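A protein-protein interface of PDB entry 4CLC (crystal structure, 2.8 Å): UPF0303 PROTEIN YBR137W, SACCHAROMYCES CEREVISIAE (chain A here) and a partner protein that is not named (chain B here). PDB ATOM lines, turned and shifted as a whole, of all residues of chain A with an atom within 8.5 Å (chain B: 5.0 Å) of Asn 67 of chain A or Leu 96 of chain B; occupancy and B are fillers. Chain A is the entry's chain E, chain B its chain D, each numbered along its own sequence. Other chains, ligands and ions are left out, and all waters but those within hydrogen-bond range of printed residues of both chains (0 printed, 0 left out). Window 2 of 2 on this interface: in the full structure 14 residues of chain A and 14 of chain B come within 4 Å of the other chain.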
ATOM      1  N   SER A  64      33.861  28.556 -20.310  1.00  0.00           N
ATOM      2  CA  SER A  64      33.547  28.189 -21.681  1.00  0.00           C
ATOM      3  C   SER A  64      32.317  28.917 -22.186  1.00  0.00           C
ATOM      4  O   SER A  64      31.459  29.285 -21.407  1.00  0.00           O
ATOM      5  CB  SER A  64      33.333  26.683 -21.788  1.00  0.00           C
ATOM      6  OG  SER A  64      34.497  25.977 -21.406  1.00  0.00           O
ATOM      7  N   LEU A  65      32.231  29.111 -23.495  1.00  0.00           N
ATOM      8  CA  LEU A  65      31.083  29.773 -24.108  1.00  0.00           C
ATOM      9  C   LEU A  65      29.906  28.823 -24.113  1.00  0.00           C
ATOM     10  O   LEU A  65      30.075  27.650 -23.844  1.00  0.00           O
ATOM     11  CB  LEU A  65      31.415  30.234 -25.531  1.00  0.00           C
ATOM     12  CG  LEU A  65      32.502  31.307 -25.628  1.00  0.00           C
ATOM     13  CD1 LEU A  65      32.503  31.917 -27.001  1.00  0.00           C
ATOM     14  CD2 LEU A  65      32.344  32.382 -24.547  1.00  0.00           C
ATOM     15  N   PRO A  66      28.696  29.326 -24.389  1.00  0.00           N
ATOM     16  CA  PRO A  66      27.557  28.400 -24.423  1.00  0.00           C
ATOM     17  C   PRO A  66      27.607  27.411 -25.575  1.00  0.00           C
ATOM     18  O   PRO A  66      26.929  26.406 -25.517  1.00  0.00           O
ATOM     19  CB  PRO A  66      26.348  29.336 -24.552  1.00  0.00           C
ATOM     20  CG  PRO A  66      26.891  30.660 -24.837  1.00  0.00           C
ATOM     21  CD  PRO A  66      28.251  30.721 -24.288  1.00  0.00           C
ATOM     22  N   ASN A  67      28.396  27.697 -26.598  1.00  0.00           N
ATOM     23  CA  ASN A  67      28.581  26.788 -27.711  1.00  0.00           C
ATOM     24  C   ASN A  67      29.785  25.840 -27.484  1.00  0.00           C
ATOM     25  O   ASN A  67      30.178  25.068 -28.360  1.00  0.00           O
ATOM     26  CB  ASN A  67      28.772  27.582 -28.986  1.00  0.00           C
ATOM     27  CG  ASN A  67      30.209  28.071 -29.158  1.00  0.00           C
ATOM     28  OD1 ASN A  67      30.878  28.465 -28.190  1.00  0.00           O
ATOM     29  ND2 ASN A  67      30.698  28.022 -30.396  1.00  0.00           N
ATOM     30  N   GLY A  68      30.381  25.928 -26.304  1.00  0.00           N
ATOM     31  CA  GLY A  68      31.340  24.935 -25.888  1.00  0.00           C
ATOM     32  C   GLY A  68      32.782  25.371 -26.027  1.00  0.00           C
ATOM     33  O   GLY A  68      33.684  24.723 -25.495  1.00  0.00           O
ATOM     34  N   HIS A  69      33.007  26.467 -26.742  1.00  0.00           N
ATOM     35  CA  HIS A  69      34.353  26.961 -26.957  1.00  0.00           C
ATOM     36  C   HIS A  69      34.993  27.295 -25.618  1.00  0.00           C
ATOM     37  O   HIS A  69      34.440  28.047 -24.841  1.00  0.00           O
ATOM     38  CB  HIS A  69      34.333  28.187 -27.867  1.00  0.00           C
ATOM     39  CG  HIS A  69      35.671  28.835 -28.030  1.00  0.00           C
ATOM     40  ND1 HIS A  69      35.873  30.188 -27.855  1.00  0.00           N
ATOM     41  CD2 HIS A  69      36.884  28.309 -28.332  1.00  0.00           C
ATOM     42  CE1 HIS A  69      37.150  30.469 -28.057  1.00  0.00           C
ATOM     43  NE2 HIS A  69      37.785  29.347 -28.343  1.00  0.00           N
ATOM     44  N   CYS A  70      36.167  26.737 -25.360  1.00  0.00           N
ATOM     45  CA  CYS A  70      36.812  26.888 -24.061  1.00  0.00           C
ATOM     46  C   CYS A  70      37.792  28.062 -24.025  1.00  0.00           C
ATOM     47  O   CYS A  70      38.717  28.127 -24.833  1.00  0.00           O
ATOM     48  CB  CYS A  70      37.533  25.592 -23.683  1.00  0.00           C
ATOM     49  SG  CYS A  70      38.469  25.696 -22.153  1.00  0.00           S
ATOM     50  N   LEU A  71      37.533  29.023 -23.147  1.00  0.00           N
ATOM     51  CA  LEU A  71      38.432  30.165 -22.957  1.00  0.00           C
ATOM     52  C   LEU A  71      39.537  29.896 -21.928  1.00  0.00           C
ATOM     53  O   LEU A  71      40.699  30.272 -22.096  1.00  0.00           O
ATOM     54  CB  LEU A  71      37.628  31.413 -22.573  1.00  0.00           C
ATOM     55  CG  LEU A  71      36.502  31.717 -23.582  1.00  0.00           C
ATOM     56  CD1 LEU A  71      35.710  32.942 -23.192  1.00  0.00           C
ATOM     57  CD2 LEU A  71      37.023  31.851 -24.991  1.00  0.00           C
ATOM     58  N   LYS A  92      28.806  21.560 -16.656  1.00  0.00           N
ATOM     59  CA  LYS A  92      28.626  22.697 -17.540  1.00  0.00           C
ATOM     60  C   LYS A  92      27.459  22.439 -18.491  1.00  0.00           C
ATOM     61  O   LYS A  92      26.673  23.334 -18.807  1.00  0.00           O
ATOM     62  CB  LYS A  92      29.919  22.948 -18.289  1.00  0.00           C
ATOM     63  CG  LYS A  92      29.867  23.957 -19.386  1.00  0.00           C
ATOM     64  CD  LYS A  92      31.239  24.077 -20.067  1.00  0.00           C
ATOM     65  CE  LYS A  92      31.623  22.783 -20.785  1.00  0.00           C
ATOM     66  NZ  LYS A  92      32.987  22.865 -21.371  1.00  0.00           N
ATOM     67  N   LEU A  96      24.043  24.915 -18.844  1.00  0.00           N
ATOM     68  CA  LEU A  96      23.692  25.563 -20.101  1.00  0.00           C
ATOM     69  C   LEU A  96      22.307  25.145 -20.623  1.00  0.00           C
ATOM     70  O   LEU A  96      21.531  25.999 -21.064  1.00  0.00           O
ATOM     71  CB  LEU A  96      24.769  25.297 -21.137  1.00  0.00           C
ATOM     72  CG  LEU A  96      26.141  25.874 -20.782  1.00  0.00           C
ATOM     73  CD1 LEU A  96      27.188  25.296 -21.720  1.00  0.00           C
ATOM     74  CD2 LEU A  96      26.138  27.389 -20.854  1.00  0.00           C
ATOM     75  N   PRO A 142      23.151  34.111 -20.794  1.00  0.00           N
ATOM     76  CA  PRO A 142      24.486  34.150 -20.192  1.00  0.00           C
ATOM     77  C   PRO A 142      25.597  34.378 -21.201  1.00  0.00           C
ATOM     78  O   PRO A 142      25.511  33.869 -22.316  1.00  0.00           O
ATOM     79  CB  PRO A 142      24.618  32.762 -19.559  1.00  0.00           C
ATOM     80  CG  PRO A 142      23.767  31.905 -20.387  1.00  0.00           C
ATOM     81  CD  PRO A 142      22.579  32.755 -20.748  1.00  0.00           C
ATOM     82  N   TYR A 143      26.621  35.130 -20.804  1.00  0.00           N
ATOM     83  CA  TYR A 143      27.824  35.288 -21.609  1.00  0.00           C
ATOM     84  C   TYR A 143      28.459  33.936 -21.845  1.00  0.00           C
ATOM     85  O   TYR A 143      28.708  33.529 -22.989  1.00  0.00           O
ATOM     86  CB  TYR A 143      28.838  36.206 -20.919  1.00  0.00           C
ATOM     87  CG  TYR A 143      28.575  37.696 -21.063  1.00  0.00           C
ATOM     88  CD1 TYR A 143      28.050  38.225 -22.224  1.00  0.00           C
ATOM     89  CD2 TYR A 143      28.859  38.563 -20.024  1.00  0.00           C
ATOM     90  CE1 TYR A 143      27.822  39.570 -22.339  1.00  0.00           C
ATOM     91  CE2 TYR A 143      28.639  39.900 -20.130  1.00  0.00           C
ATOM     92  CZ  TYR A 143      28.120  40.408 -21.282  1.00  0.00           C
ATOM     93  OH  TYR A 143      27.897  41.774 -21.375  1.00  0.00           O
ATOM     94  N   ALA A 144      28.698  33.243 -20.736  1.00  0.00           N
ATOM     95  CA  ALA A 144      29.454  32.001 -20.726  1.00  0.00           C
ATOM     96  C   ALA A 144      29.212  31.253 -19.420  1.00  0.00           C
ATOM     97  O   ALA A 144      28.444  31.702 -18.573  1.00  0.00           O
ATOM     98  CB  ALA A 144      30.942  32.289 -20.916  1.00  0.00           C
ATOM     99  N   CYS A 145      29.873  30.114 -19.259  1.00  0.00           N
ATOM    100  CA  CYS A 145      29.739  29.324 -18.048  1.00  0.00           C
ATOM    101  C   CYS A 145      31.042  29.234 -17.279  1.00  0.00           C
ATOM    102  O   CYS A 145      32.132  29.249 -17.862  1.00  0.00           O
ATOM    103  CB  CYS A 145      29.255  27.926 -18.378  1.00  0.00           C
ATOM    104  SG  CYS A 145      28.912  26.922 -16.925  1.00  0.00           S
ATOM    105  N   LEU B  65      20.400  30.782 -29.831  1.00  0.00           N
ATOM    106  CA  LEU B  65      21.570  31.076 -29.040  1.00  0.00           C
ATOM    107  C   LEU B  65      22.664  30.154 -29.516  1.00  0.00           C
ATOM    108  O   LEU B  65      22.380  29.189 -30.221  1.00  0.00           O
ATOM    109  CB  LEU B  65      21.282  30.887 -27.560  1.00  0.00           C
ATOM    110  CG  LEU B  65      20.240  31.800 -26.945  1.00  0.00           C
ATOM    111  CD1 LEU B  65      20.165  31.547 -25.458  1.00  0.00           C
ATOM    112  CD2 LEU B  65      20.607  33.232 -27.231  1.00  0.00           C
ATOM    113  N   PRO B  66      23.925  30.447 -29.155  1.00  0.00           N
ATOM    114  CA  PRO B  66      25.025  29.576 -29.566  1.00  0.00           C
ATOM    115  C   PRO B  66      24.909  28.176 -29.009  1.00  0.00           C
ATOM    116  O   PRO B  66      25.528  27.265 -29.550  1.00  0.00           O
ATOM    117  CB  PRO B  66      26.264  30.274 -29.003  1.00  0.00           C
ATOM    118  CG  PRO B  66      25.755  31.287 -28.059  1.00  0.00           C
ATOM    119  CD  PRO B  66      24.418  31.678 -28.520  1.00  0.00           C
ATOM    120  N   ASN B  67      24.131  28.010 -27.942  1.00  0.00           N
ATOM    121  CA  ASN B  67      23.957  26.711 -27.327  1.00  0.00           C
ATOM    122  C   ASN B  67      22.870  25.880 -28.021  1.00  0.00           C
ATOM    123  O   ASN B  67      22.690  24.706 -27.712  1.00  0.00           O
ATOM    124  CB  ASN B  67      23.647  26.886 -25.843  1.00  0.00           C
ATOM    125  CG  ASN B  67      22.184  27.158 -25.584  1.00  0.00           C
ATOM    126  OD1 ASN B  67      21.476  27.721 -26.423  1.00  0.00           O
ATOM    127  ND2 ASN B  67      21.712  26.733 -24.422  1.00  0.00           N
ATOM    128  N   LYS B  92      23.815  27.761 -39.580  1.00  0.00           N
ATOM    129  CA  LYS B  92      24.006  28.189 -38.195  1.00  0.00           C
ATOM    130  C   LYS B  92      25.206  27.492 -37.593  1.00  0.00           C
ATOM    131  O   LYS B  92      26.024  28.113 -36.919  1.00  0.00           O
ATOM    132  CB  LYS B  92      22.746  27.891 -37.366  1.00  0.00           C
ATOM    133  CG  LYS B  92      22.837  28.303 -35.919  1.00  0.00           C
ATOM    134  CD  LYS B  92      21.561  28.042 -35.148  1.00  0.00           C
ATOM    135  CE  LYS B  92      21.155  26.606 -35.192  1.00  0.00           C
ATOM    136  NZ  LYS B  92      19.799  26.507 -35.788  1.00  0.00           N
ATOM    137  N   LYS B  93      25.310  26.196 -37.858  1.00  0.00           N
ATOM    138  CA  LYS B  93      26.379  25.406 -37.292  1.00  0.00           C
ATOM    139  C   LYS B  93      27.731  25.958 -37.741  1.00  0.00           C
ATOM    140  O   LYS B  93      28.596  26.256 -36.904  1.00  0.00           O
ATOM    141  CB  LYS B  93      26.232  23.923 -37.663  1.00  0.00           C
ATOM    142  CG  LYS B  93      27.099  23.048 -36.776  1.00  0.00           C
ATOM    143  CD  LYS B  93      26.823  21.568 -36.899  1.00  0.00           C
ATOM    144  CE  LYS B  93      27.607  20.789 -35.835  1.00  0.00           C
ATOM    145  NZ  LYS B  93      27.010  19.452 -35.511  1.00  0.00           N
ATOM    146  N   THR B  94      27.903  26.114 -39.055  1.00  0.00           N
ATOM    147  CA  THR B  94      29.119  26.709 -39.597  1.00  0.00           C
ATOM    148  C   THR B  94      29.407  28.056 -38.942  1.00  0.00           C
ATOM    149  O   THR B  94      30.474  28.243 -38.361  1.00  0.00           O
ATOM    150  CB  THR B  94      29.035  26.920 -41.111  1.00  0.00           C
ATOM    151  OG1 THR B  94      28.894  25.665 -41.794  1.00  0.00           O
ATOM    152  CG2 THR B  94      30.269  27.613 -41.583  1.00  0.00           C
ATOM    153  N   ALA B  95      28.446  28.976 -38.997  1.00  0.00           N
ATOM    154  CA  ALA B  95      28.628  30.311 -38.424  1.00  0.00           C
ATOM    155  C   ALA B  95      29.066  30.333 -36.961  1.00  0.00           C
ATOM    156  O   ALA B  95      29.986  31.072 -36.622  1.00  0.00           O
ATOM    157  CB  ALA B  95      27.366  31.109 -38.575  1.00  0.00           C
ATOM    158  N   LEU B  96      28.425  29.545 -36.092  1.00  0.00           N
ATOM    159  CA  LEU B  96      28.743  29.583 -34.655  1.00  0.00           C
ATOM    160  C   LEU B  96      30.110  28.982 -34.369  1.00  0.00           C
ATOM    161  O   LEU B  96      30.816  29.388 -33.434  1.00  0.00           O
ATOM    162  CB  LEU B  96      27.670  28.860 -33.836  1.00  0.00           C
ATOM    163  CG  LEU B  96      26.342  29.602 -33.628  1.00  0.00           C
ATOM    164  CD1 LEU B  96      25.225  28.628 -33.244  1.00  0.00           C
ATOM    165  CD2 LEU B  96      26.473  30.731 -32.607  1.00  0.00           C
ATOM    166  N   ARG B  97      30.488  28.013 -35.185  1.00  0.00           N
ATOM    167  CA  ARG B  97      31.764  27.351 -35.007  1.00  0.00           C
ATOM    168  C   ARG B  97      32.934  28.224 -35.436  1.00  0.00           C
ATOM    169  O   ARG B  97      33.954  28.320 -34.732  1.00  0.00           O
ATOM    170  CB  ARG B  97      31.804  26.046 -35.796  1.00  0.00           C
ATOM    171  CG  ARG B  97      33.172  25.438 -35.821  1.00  0.00           C
ATOM    172  CD  ARG B  97      33.172  24.064 -36.441  1.00  0.00           C
ATOM    173  NE  ARG B  97      34.533  23.526 -36.507  1.00  0.00           N
ATOM    174  CZ  ARG B  97      34.820  22.259 -36.770  1.00  0.00           C
ATOM    175  NH1 ARG B  97      33.840  21.387 -36.981  1.00  0.00           N
ATOM    176  NH2 ARG B  97      36.083  21.865 -36.809  1.00  0.00           N
ATOM    177  N   PHE B  98      32.804  28.831 -36.615  1.00  0.00           N
ATOM    178  CA  PHE B  98      33.947  29.497 -37.214  1.00  0.00           C
ATOM    179  C   PHE B  98      34.068  30.979 -36.879  1.00  0.00           C
ATOM    180  O   PHE B  98      35.135  31.568 -37.074  1.00  0.00           O
ATOM    181  CB  PHE B  98      33.910  29.282 -38.713  1.00  0.00           C
ATOM    182  CG  PHE B  98      34.186  27.850 -39.122  1.00  0.00           C
ATOM    183  CD1 PHE B  98      35.481  27.360 -39.145  1.00  0.00           C
ATOM    184  CD2 PHE B  98      33.148  27.002 -39.480  1.00  0.00           C
ATOM    185  CE1 PHE B  98      35.732  26.044 -39.522  1.00  0.00           C
ATOM    186  CE2 PHE B  98      33.387  25.703 -39.854  1.00  0.00           C
ATOM    187  CZ  PHE B  98      34.686  25.220 -39.879  1.00  0.00           C
ATOM    188  N   GLY B  99      33.007  31.556 -36.322  1.00  0.00           N
ATOM    189  CA  GLY B  99      33.013  32.956 -35.938  1.00  0.00           C
ATOM    190  C   GLY B  99      32.780  33.969 -37.058  1.00  0.00           C
ATOM    191  O   GLY B  99      33.053  35.160 -36.879  1.00  0.00           O
ATOM    192  N   LEU B 133      26.028  35.898 -37.463  1.00  0.00           N
ATOM    193  CA  LEU B 133      26.076  36.024 -36.031  1.00  0.00           C
ATOM    194  C   LEU B 133      25.538  37.380 -35.599  1.00  0.00           C
ATOM    195  O   LEU B 133      25.637  38.360 -36.340  1.00  0.00           O
ATOM    196  CB  LEU B 133      27.504  35.836 -35.520  1.00  0.00           C
ATOM    197  CG  LEU B 133      28.119  34.459 -35.739  1.00  0.00           C
ATOM    198  CD1 LEU B 133      29.596  34.492 -35.406  1.00  0.00           C
ATOM    199  CD2 LEU B 133      27.416  33.450 -34.888  1.00  0.00           C
ATOM    200  N   ALA B 144      24.046  35.692 -30.377  1.00  0.00           N
ATOM    201  CA  ALA B 144      23.206  34.703 -31.015  1.00  0.00           C
ATOM    202  C   ALA B 144      23.602  34.587 -32.472  1.00  0.00           C
ATOM    203  O   ALA B 144      24.633  35.084 -32.878  1.00  0.00           O
ATOM    204  CB  ALA B 144      21.750  35.081 -30.880  1.00  0.00           C
ATOM    205  N   CYS B 145      22.790  33.895 -33.250  1.00  0.00           N
ATOM    206  CA  CYS B 145      23.015  33.799 -34.667  1.00  0.00           C
ATOM    207  C   CYS B 145      21.664  33.956 -35.379  1.00  0.00           C
ATOM    208  O   CYS B 145      20.656  33.349 -34.991  1.00  0.00           O
ATOM    209  CB  CYS B 145      23.703  32.470 -35.004  1.00  0.00           C
ATOM    210  SG  CYS B 145      23.937  32.104 -36.767  1.00  0.00           S
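Among the printed residues, merely in contact across the chains: Asn 67 of chain A with Pro 66 of chain B, Pro 66 of chain A with Asn 67 of chain B and Pro 66 of chain A with Pro 66 of chain B.
Hydrophobic or aromatic side chains of chain B within 4 Å of the printed part of chain A: Pro 66. Hydrophobic or aromatic side chains of chain A that line the printed part of chain B: Pro 66. Among the printed residues, 5 pairs touch across the chains.
The side-chain amide oxygen (OD1) of Asn 67 of chain A lies within hydrogen-bond range of the backbone NH (N) of His 69 of chain A, 3.3 Å away.
Of the printed residues of chain B, Pro 66 of chain A touches Pro 66 (3.5 Å) and Asn 67 (3.3 Å). Asn 67 of chain A touches just these residues of chain B: Pro 66 (3.3 Å) and Leu 96 (3.3 Å). Of the printed residues of chain B, Leu 96 of chain A touches Asn 67. Of the printed residues of chain A, Pro 66 of chain B touches Pro 66 (3.5 Å) and Asn 67 (3.3 Å). Of the printed residues of chain A, Asn 67 of chain B touches Pro 66 and Leu 96. Thr 94 of chain B touches none of the printed residues of chain A. No residue of chain A comes within 4 Å of Ala 95 of chain B. Printed residues of chain A within 4 Å of Leu 96 of chain B: Asn 67. The nearest residue of chain B that does not touch Asn 67 of chain A is Asn 67 of chain B (4.5 Å). The nearest residue of chain A that does not touch Leu 96 of chain B is His 69 of chain A (6.7 Å).
The side-chain amide nitrogen (ND2) of Asn 67 of chain A lies within hydrogen-bond range of the backbone carbonyl oxygen (O) of Leu 96 of chain B (3.3 Å). ND2 of Asn 67 of chain B lies within hydrogen-bond range of O of Leu 96 of chain A (3.4 Å).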
